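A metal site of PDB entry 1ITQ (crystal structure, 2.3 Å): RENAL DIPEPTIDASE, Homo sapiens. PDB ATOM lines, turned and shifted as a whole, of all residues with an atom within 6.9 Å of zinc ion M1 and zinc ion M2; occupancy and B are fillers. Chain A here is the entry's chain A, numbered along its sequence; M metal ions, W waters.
Merely in contact with zinc ion M1: Ser 66 (3.9 Å) and Asp 288 (3.9 Å).
Zinc ion M1 is bound by a ring nitrogen (NE2) of His 20 (2.0 Å), water W3 (2.2 Å), the side-chain carboxylate of Asp 22 (2.3 Å) and the side-chain carboxylate of Glu 125 (2.4 Å). Slightly farther from zinc ion M1 lies water W2 (2.8 Å). Slightly farther from zinc ion M1 lies the side-chain carboxylate (OD2) of Asp 22 (2.8 Å).
Merely in contact with zinc ion M2: Arg 230 (3.99 Å). Within 4 Å of zinc ion M2: His 20, Glu 125, His 198, His 219 and Arg 230. The nearest printed residue that does not touch zinc ion M2 is His 152 (4.2 Å).
Water W1 lies within hydrogen-bond range of the side-chain carboxylate (OD2) of Asp 288 and the guanidinium group (NH1) of Arg 230.
Zinc ion M2 is bound by a ring nitrogen (NE2) of His 219 (2.1 Å), the side-chain carboxylate of Glu 125 (2.3 Å) and a ring nitrogen (NE2) of His 198 (2.3 Å). Zinc ion M2 has three donor atoms within binding distance. Slightly farther from zinc ion M2 lies water W1 (2.6 Å). Slightly farther from zinc ion M2 lies water W2 (2.8 Å).
ND1 of His 198 is in hydrogen-bond range of OG of Ser 153 (3.5 Å). The backbone carbonyl oxygen of His 20 lies within hydrogen-bond range of the backbone NH of Asp 288, at 3.0 Å. ND1 of His 20 sits at hydrogen-bond distance from OH of Tyr 147 (2.8 Å). A ring nitrogen (ND1) of His 219 sits at hydrogen-bond distance from the side-chain hydroxyl (OG) of Ser 218. A ring nitrogen (ND1) of His 20 sits close to a ring nitrogen (ND1) of His 219, at 3.4 Å. OD2 of Asp 288 is in hydrogen-bond range of ND2 of Asn 250. The backbone carbonyl oxygen (O) of His 219 sits at hydrogen-bond distance from the guanidinium group (NH1) of Arg 230, at 2.6 Å. The side-chain carboxylate (OD2) of Asp 22 sits at hydrogen-bond distance from the side-chain hydroxyl (OG) of Ser 66, at 2.8 Å.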
ATOM      1  N   HIS A  20     -23.760   8.048  25.179  1.00  0.00           N
ATOM      2  CA  HIS A  20     -23.489   6.733  24.603  1.00  0.00           C
ATOM      3  C   HIS A  20     -23.374   6.665  23.074  1.00  0.00           C
ATOM      4  O   HIS A  20     -24.371   6.690  22.365  1.00  0.00           O
ATOM      5  CB  HIS A  20     -24.554   5.753  25.064  1.00  0.00           C
ATOM      6  CG  HIS A  20     -24.231   4.323  24.775  1.00  0.00           C
ATOM      7  ND1 HIS A  20     -23.475   3.527  25.611  1.00  0.00           N
ATOM      8  CD2 HIS A  20     -24.565   3.538  23.722  1.00  0.00           C
ATOM      9  CE1 HIS A  20     -23.394   2.317  25.043  1.00  0.00           C
ATOM     10  NE2 HIS A  20     -24.035   2.284  23.896  1.00  0.00           N
ATOM     11  N   ASN A  21     -22.147   6.519  22.576  1.00  0.00           N
ATOM     12  CA  ASN A  21     -21.899   6.396  21.138  1.00  0.00           C
ATOM     13  C   ASN A  21     -21.078   5.131  20.871  1.00  0.00           C
ATOM     14  O   ASN A  21     -19.977   4.975  21.416  1.00  0.00           O
ATOM     15  CB  ASN A  21     -21.183   7.615  20.581  1.00  0.00           C
ATOM     16  CG  ASN A  21     -21.064   7.561  19.072  1.00  0.00           C
ATOM     17  OD1 ASN A  21     -20.585   6.577  18.501  1.00  0.00           O
ATOM     18  ND2 ASN A  21     -21.520   8.612  18.405  1.00  0.00           N
ATOM     19  N   ASP A  22     -21.595   4.275  19.994  1.00  0.00           N
ATOM     20  CA  ASP A  22     -20.948   3.021  19.681  1.00  0.00           C
ATOM     21  C   ASP A  22     -20.041   2.994  18.476  1.00  0.00           C
ATOM     22  O   ASP A  22     -19.995   1.990  17.762  1.00  0.00           O
ATOM     23  CB  ASP A  22     -21.973   1.919  19.551  1.00  0.00           C
ATOM     24  CG  ASP A  22     -22.492   1.472  20.886  1.00  0.00           C
ATOM     25  OD1 ASP A  22     -23.666   1.775  21.186  1.00  0.00           O
ATOM     26  OD2 ASP A  22     -21.724   0.826  21.631  1.00  0.00           O
ATOM     27  N   SER A  66     -18.553   4.397  23.959  1.00  0.00           N
ATOM     28  CA  SER A  66     -18.916   3.094  24.451  1.00  0.00           C
ATOM     29  C   SER A  66     -17.922   1.991  24.123  1.00  0.00           C
ATOM     30  O   SER A  66     -17.651   1.712  22.962  1.00  0.00           O
ATOM     31  CB  SER A  66     -20.291   2.717  23.894  1.00  0.00           C
ATOM     32  OG  SER A  66     -20.581   1.369  24.164  1.00  0.00           O
ATOM     33  N   TYR A  68     -17.755  -1.485  24.101  1.00  0.00           N
ATOM     34  CA  TYR A  68     -18.714  -2.562  24.096  1.00  0.00           C
ATOM     35  C   TYR A  68     -18.243  -3.850  23.461  1.00  0.00           C
ATOM     36  O   TYR A  68     -17.581  -3.844  22.428  1.00  0.00           O
ATOM     37  CB  TYR A  68     -19.981  -2.051  23.374  1.00  0.00           C
ATOM     38  CG  TYR A  68     -20.930  -3.127  22.924  1.00  0.00           C
ATOM     39  CD1 TYR A  68     -20.983  -3.519  21.595  1.00  0.00           C
ATOM     40  CD2 TYR A  68     -21.751  -3.788  23.833  1.00  0.00           C
ATOM     41  CE1 TYR A  68     -21.825  -4.543  21.176  1.00  0.00           C
ATOM     42  CE2 TYR A  68     -22.593  -4.800  23.447  1.00  0.00           C
ATOM     43  CZ  TYR A  68     -22.630  -5.178  22.119  1.00  0.00           C
ATOM     44  OH  TYR A  68     -23.468  -6.209  21.745  1.00  0.00           O
ATOM     45  N   GLU A 125     -19.968  -0.743  28.560  1.00  0.00           N
ATOM     46  CA  GLU A 125     -21.320  -1.250  28.490  1.00  0.00           C
ATOM     47  C   GLU A 125     -21.523  -2.739  28.702  1.00  0.00           C
ATOM     48  O   GLU A 125     -21.511  -3.524  27.745  1.00  0.00           O
ATOM     49  CB  GLU A 125     -21.965  -0.834  27.170  1.00  0.00           C
ATOM     50  CG  GLU A 125     -23.397  -1.256  27.079  1.00  0.00           C
ATOM     51  CD  GLU A 125     -24.023  -0.857  25.777  1.00  0.00           C
ATOM     52  OE1 GLU A 125     -23.320  -0.850  24.750  1.00  0.00           O
ATOM     53  OE2 GLU A 125     -25.228  -0.558  25.793  1.00  0.00           O
ATOM     54  N   TYR A 147     -17.904   4.952  33.621  1.00  0.00           N
ATOM     55  CA  TYR A 147     -19.280   4.519  33.819  1.00  0.00           C
ATOM     56  C   TYR A 147     -19.333   3.076  33.414  1.00  0.00           C
ATOM     57  O   TYR A 147     -18.560   2.646  32.561  1.00  0.00           O
ATOM     58  CB  TYR A 147     -20.348   5.431  33.152  1.00  0.00           C
ATOM     59  CG  TYR A 147     -20.793   5.212  31.707  1.00  0.00           C
ATOM     60  CD1 TYR A 147     -21.171   3.966  31.219  1.00  0.00           C
ATOM     61  CD2 TYR A 147     -20.912   6.309  30.847  1.00  0.00           C
ATOM     62  CE1 TYR A 147     -21.660   3.814  29.904  1.00  0.00           C
ATOM     63  CE2 TYR A 147     -21.393   6.160  29.542  1.00  0.00           C
ATOM     64  CZ  TYR A 147     -21.762   4.937  29.078  1.00  0.00           C
ATOM     65  OH  TYR A 147     -22.241   4.820  27.781  1.00  0.00           O
ATOM     66  N   THR A 149     -22.155   0.129  32.623  1.00  0.00           N
ATOM     67  CA  THR A 149     -23.540  -0.232  32.432  1.00  0.00           C
ATOM     68  C   THR A 149     -23.570  -1.605  33.098  1.00  0.00           C
ATOM     69  O   THR A 149     -23.025  -2.570  32.544  1.00  0.00           O
ATOM     70  CB  THR A 149     -23.872  -0.358  30.937  1.00  0.00           C
ATOM     71  OG1 THR A 149     -23.426   0.811  30.251  1.00  0.00           O
ATOM     72  CG2 THR A 149     -25.357  -0.496  30.734  1.00  0.00           C
ATOM     73  N   HIS A 152     -25.883  -5.614  30.010  1.00  0.00           N
ATOM     74  CA  HIS A 152     -26.225  -5.301  28.650  1.00  0.00           C
ATOM     75  C   HIS A 152     -27.487  -6.115  28.426  1.00  0.00           C
ATOM     76  O   HIS A 152     -28.338  -6.180  29.308  1.00  0.00           O
ATOM     77  CB  HIS A 152     -25.113  -5.721  27.695  1.00  0.00           C
ATOM     78  CG  HIS A 152     -25.306  -5.184  26.328  1.00  0.00           C
ATOM     79  ND1 HIS A 152     -25.767  -5.955  25.283  1.00  0.00           N
ATOM     80  CD2 HIS A 152     -25.161  -3.926  25.839  1.00  0.00           C
ATOM     81  CE1 HIS A 152     -25.902  -5.195  24.212  1.00  0.00           C
ATOM     82  NE2 HIS A 152     -25.548  -3.963  24.522  1.00  0.00           N
ATOM     83  N   SER A 153     -27.617  -6.752  27.275  1.00  0.00           N
ATOM     84  CA  SER A 153     -28.817  -7.539  27.023  1.00  0.00           C
ATOM     85  C   SER A 153     -28.681  -8.967  27.517  1.00  0.00           C
ATOM     86  O   SER A 153     -29.099  -9.916  26.841  1.00  0.00           O
ATOM     87  CB  SER A 153     -29.202  -7.493  25.550  1.00  0.00           C
ATOM     88  OG  SER A 153     -29.689  -6.207  25.208  1.00  0.00           O
ATOM     89  N   ALA A 197     -28.775   1.769  32.167  1.00  0.00           N
ATOM     90  CA  ALA A 197     -29.342   1.446  30.871  1.00  0.00           C
ATOM     91  C   ALA A 197     -29.205  -0.069  30.738  1.00  0.00           C
ATOM     92  O   ALA A 197     -28.254  -0.648  31.253  1.00  0.00           O
ATOM     93  CB  ALA A 197     -28.572   2.145  29.780  1.00  0.00           C
ATOM     94  N   HIS A 198     -30.191  -0.706  30.125  1.00  0.00           N
ATOM     95  CA  HIS A 198     -30.171  -2.153  29.940  1.00  0.00           C
ATOM     96  C   HIS A 198     -30.526  -3.064  31.123  1.00  0.00           C
ATOM     97  O   HIS A 198     -30.708  -4.268  30.913  1.00  0.00           O
ATOM     98  CB  HIS A 198     -28.824  -2.597  29.381  1.00  0.00           C
ATOM     99  CG  HIS A 198     -28.669  -2.364  27.912  1.00  0.00           C
ATOM    100  ND1 HIS A 198     -29.149  -3.228  26.946  1.00  0.00           N
ATOM    101  CD2 HIS A 198     -28.012  -1.394  27.248  1.00  0.00           C
ATOM    102  CE1 HIS A 198     -28.752  -2.762  25.751  1.00  0.00           C
ATOM    103  NE2 HIS A 198     -28.066  -1.642  25.883  1.00  0.00           N
ATOM    104  N   SER A 218     -27.462   6.001  30.631  1.00  0.00           N
ATOM    105  CA  SER A 218     -26.682   6.601  29.536  1.00  0.00           C
ATOM    106  C   SER A 218     -27.385   6.667  28.186  1.00  0.00           C
ATOM    107  O   SER A 218     -26.990   7.440  27.334  1.00  0.00           O
ATOM    108  CB  SER A 218     -25.348   5.883  29.390  1.00  0.00           C
ATOM    109  OG  SER A 218     -25.562   4.545  29.018  1.00  0.00           O
ATOM    110  N   HIS A 219     -28.347   5.776  27.980  1.00  0.00           N
ATOM    111  CA  HIS A 219     -29.114   5.756  26.750  1.00  0.00           C
ATOM    112  C   HIS A 219     -30.469   5.056  26.932  1.00  0.00           C
ATOM    113  O   HIS A 219     -30.711   3.980  26.382  1.00  0.00           O
ATOM    114  CB  HIS A 219     -28.311   5.197  25.550  1.00  0.00           C
ATOM    115  CG  HIS A 219     -27.694   3.860  25.794  1.00  0.00           C
ATOM    116  ND1 HIS A 219     -26.695   3.622  26.713  1.00  0.00           N
ATOM    117  CD2 HIS A 219     -27.902   2.677  25.170  1.00  0.00           C
ATOM    118  CE1 HIS A 219     -26.336   2.345  26.622  1.00  0.00           C
ATOM    119  NE2 HIS A 219     -27.038   1.723  25.693  1.00  0.00           N
ATOM    120  N   ARG A 230     -36.640  -1.255  27.654  1.00  0.00           N
ATOM    121  CA  ARG A 230     -35.356  -0.603  27.568  1.00  0.00           C
ATOM    122  C   ARG A 230     -35.590   0.829  28.008  1.00  0.00           C
ATOM    123  O   ARG A 230     -34.679   1.635  28.042  1.00  0.00           O
ATOM    124  CB  ARG A 230     -34.824  -0.636  26.135  1.00  0.00           C
ATOM    125  CG  ARG A 230     -33.840  -1.756  25.892  1.00  0.00           C
ATOM    126  CD  ARG A 230     -32.601  -1.553  26.768  1.00  0.00           C
ATOM    127  NE  ARG A 230     -31.674  -0.577  26.193  1.00  0.00           N
ATOM    128  CZ  ARG A 230     -31.348   0.587  26.744  1.00  0.00           C
ATOM    129  NH1 ARG A 230     -30.488   1.383  26.137  1.00  0.00           N
ATOM    130  NH2 ARG A 230     -31.898   0.979  27.887  1.00  0.00           N
ATOM    131  N   ASN A 250     -32.302   8.004  24.515  1.00  0.00           N
ATOM    132  CA  ASN A 250     -31.894   7.162  23.398  1.00  0.00           C
ATOM    133  C   ASN A 250     -32.742   7.517  22.167  1.00  0.00           C
ATOM    134  O   ASN A 250     -33.979   7.524  22.243  1.00  0.00           O
ATOM    135  CB  ASN A 250     -32.134   5.695  23.786  1.00  0.00           C
ATOM    136  CG  ASN A 250     -31.498   4.718  22.841  1.00  0.00           C
ATOM    137  OD1 ASN A 250     -31.451   4.938  21.637  1.00  0.00           O
ATOM    138  ND2 ASN A 250     -31.011   3.594  23.380  1.00  0.00           N
ATOM    139  N   TYR A 255     -37.529   2.785  20.295  1.00  0.00           N
ATOM    140  CA  TYR A 255     -37.645   3.099  21.712  1.00  0.00           C
ATOM    141  C   TYR A 255     -38.316   4.470  21.816  1.00  0.00           C
ATOM    142  O   TYR A 255     -38.771   4.889  22.890  1.00  0.00           O
ATOM    143  CB  TYR A 255     -36.270   3.171  22.382  1.00  0.00           C
ATOM    144  CG  TYR A 255     -35.516   1.855  22.453  1.00  0.00           C
ATOM    145  CD1 TYR A 255     -36.118   0.643  22.114  1.00  0.00           C
ATOM    146  CD2 TYR A 255     -34.174   1.845  22.828  1.00  0.00           C
ATOM    147  CE1 TYR A 255     -35.406  -0.542  22.149  1.00  0.00           C
ATOM    148  CE2 TYR A 255     -33.446   0.648  22.873  1.00  0.00           C
ATOM    149  CZ  TYR A 255     -34.060  -0.531  22.522  1.00  0.00           C
ATOM    150  OH  TYR A 255     -33.314  -1.678  22.539  1.00  0.00           O
ATOM    151  N   ASP A 288     -27.218   7.004  21.320  1.00  0.00           N
ATOM    152  CA  ASP A 288     -27.019   5.624  20.880  1.00  0.00           C
ATOM    153  C   ASP A 288     -26.639   5.571  19.395  1.00  0.00           C
ATOM    154  O   ASP A 288     -26.894   4.582  18.701  1.00  0.00           O
ATOM    155  CB  ASP A 288     -28.264   4.760  21.159  1.00  0.00           C
ATOM    156  CG  ASP A 288     -27.931   3.292  21.319  1.00  0.00           C
ATOM    157  OD1 ASP A 288     -26.740   2.919  21.236  1.00  0.00           O
ATOM    158  OD2 ASP A 288     -28.876   2.492  21.527  1.00  0.00           O
ATOM    159  N   ASP A 290     -24.558   4.988  16.131  1.00  0.00           N
ATOM    160  CA  ASP A 290     -23.615   3.955  15.719  1.00  0.00           C
ATOM    161  C   ASP A 290     -23.783   2.643  16.469  1.00  0.00           C
ATOM    162  O   ASP A 290     -23.031   1.694  16.274  1.00  0.00           O
ATOM    163  CB  ASP A 290     -22.181   4.467  15.763  1.00  0.00           C
ATOM    164  CG  ASP A 290     -21.801   5.213  14.512  1.00  0.00           C
ATOM    165  OD1 ASP A 290     -22.192   4.745  13.422  1.00  0.00           O
ATOM    166  OD2 ASP A 290     -21.128   6.264  14.594  1.00  0.00           O
ATOM    167  N   GLY A 291     -24.817   2.600  17.290  1.00  0.00           N
ATOM    168  CA  GLY A 291     -25.113   1.392  18.030  1.00  0.00           C
ATOM    169  C   GLY A 291     -26.416   0.815  17.527  1.00  0.00           C
ATOM    170  O   GLY A 291     -26.648  -0.390  17.628  1.00  0.00           O
ATOM    171  N   VAL A 292     -27.269   1.691  16.975  1.00  0.00           N
ATOM    172  CA  VAL A 292     -28.580   1.307  16.445  1.00  0.00           C
ATOM    173  C   VAL A 292     -28.675   1.495  14.930  1.00  0.00           C
ATOM    174  O   VAL A 292     -28.028   2.381  14.374  1.00  0.00           O
ATOM    175  CB  VAL A 292     -29.705   2.092  17.151  1.00  0.00           C
ATOM    176  CG1 VAL A 292     -29.821   1.634  18.598  1.00  0.00           C
ATOM    177  CG2 VAL A 292     -29.433   3.592  17.093  1.00  0.00           C
HETATM  178 ZN    ZN M   1     -24.176   0.481  22.977  1.00  0.00          ZN
HETATM  179 ZN    ZN M   2     -27.084  -0.035  24.626  1.00  0.00          ZN
HETATM  180  O   HOH W   1     -29.354  -0.066  23.284  1.00  0.00           O
HETATM  181  O   HOH W   2     -26.628  -0.213  21.867  1.00  0.00           O
HETATM  182  O   HOH W   3     -24.025  -1.537  22.043  1.00  0.00           O
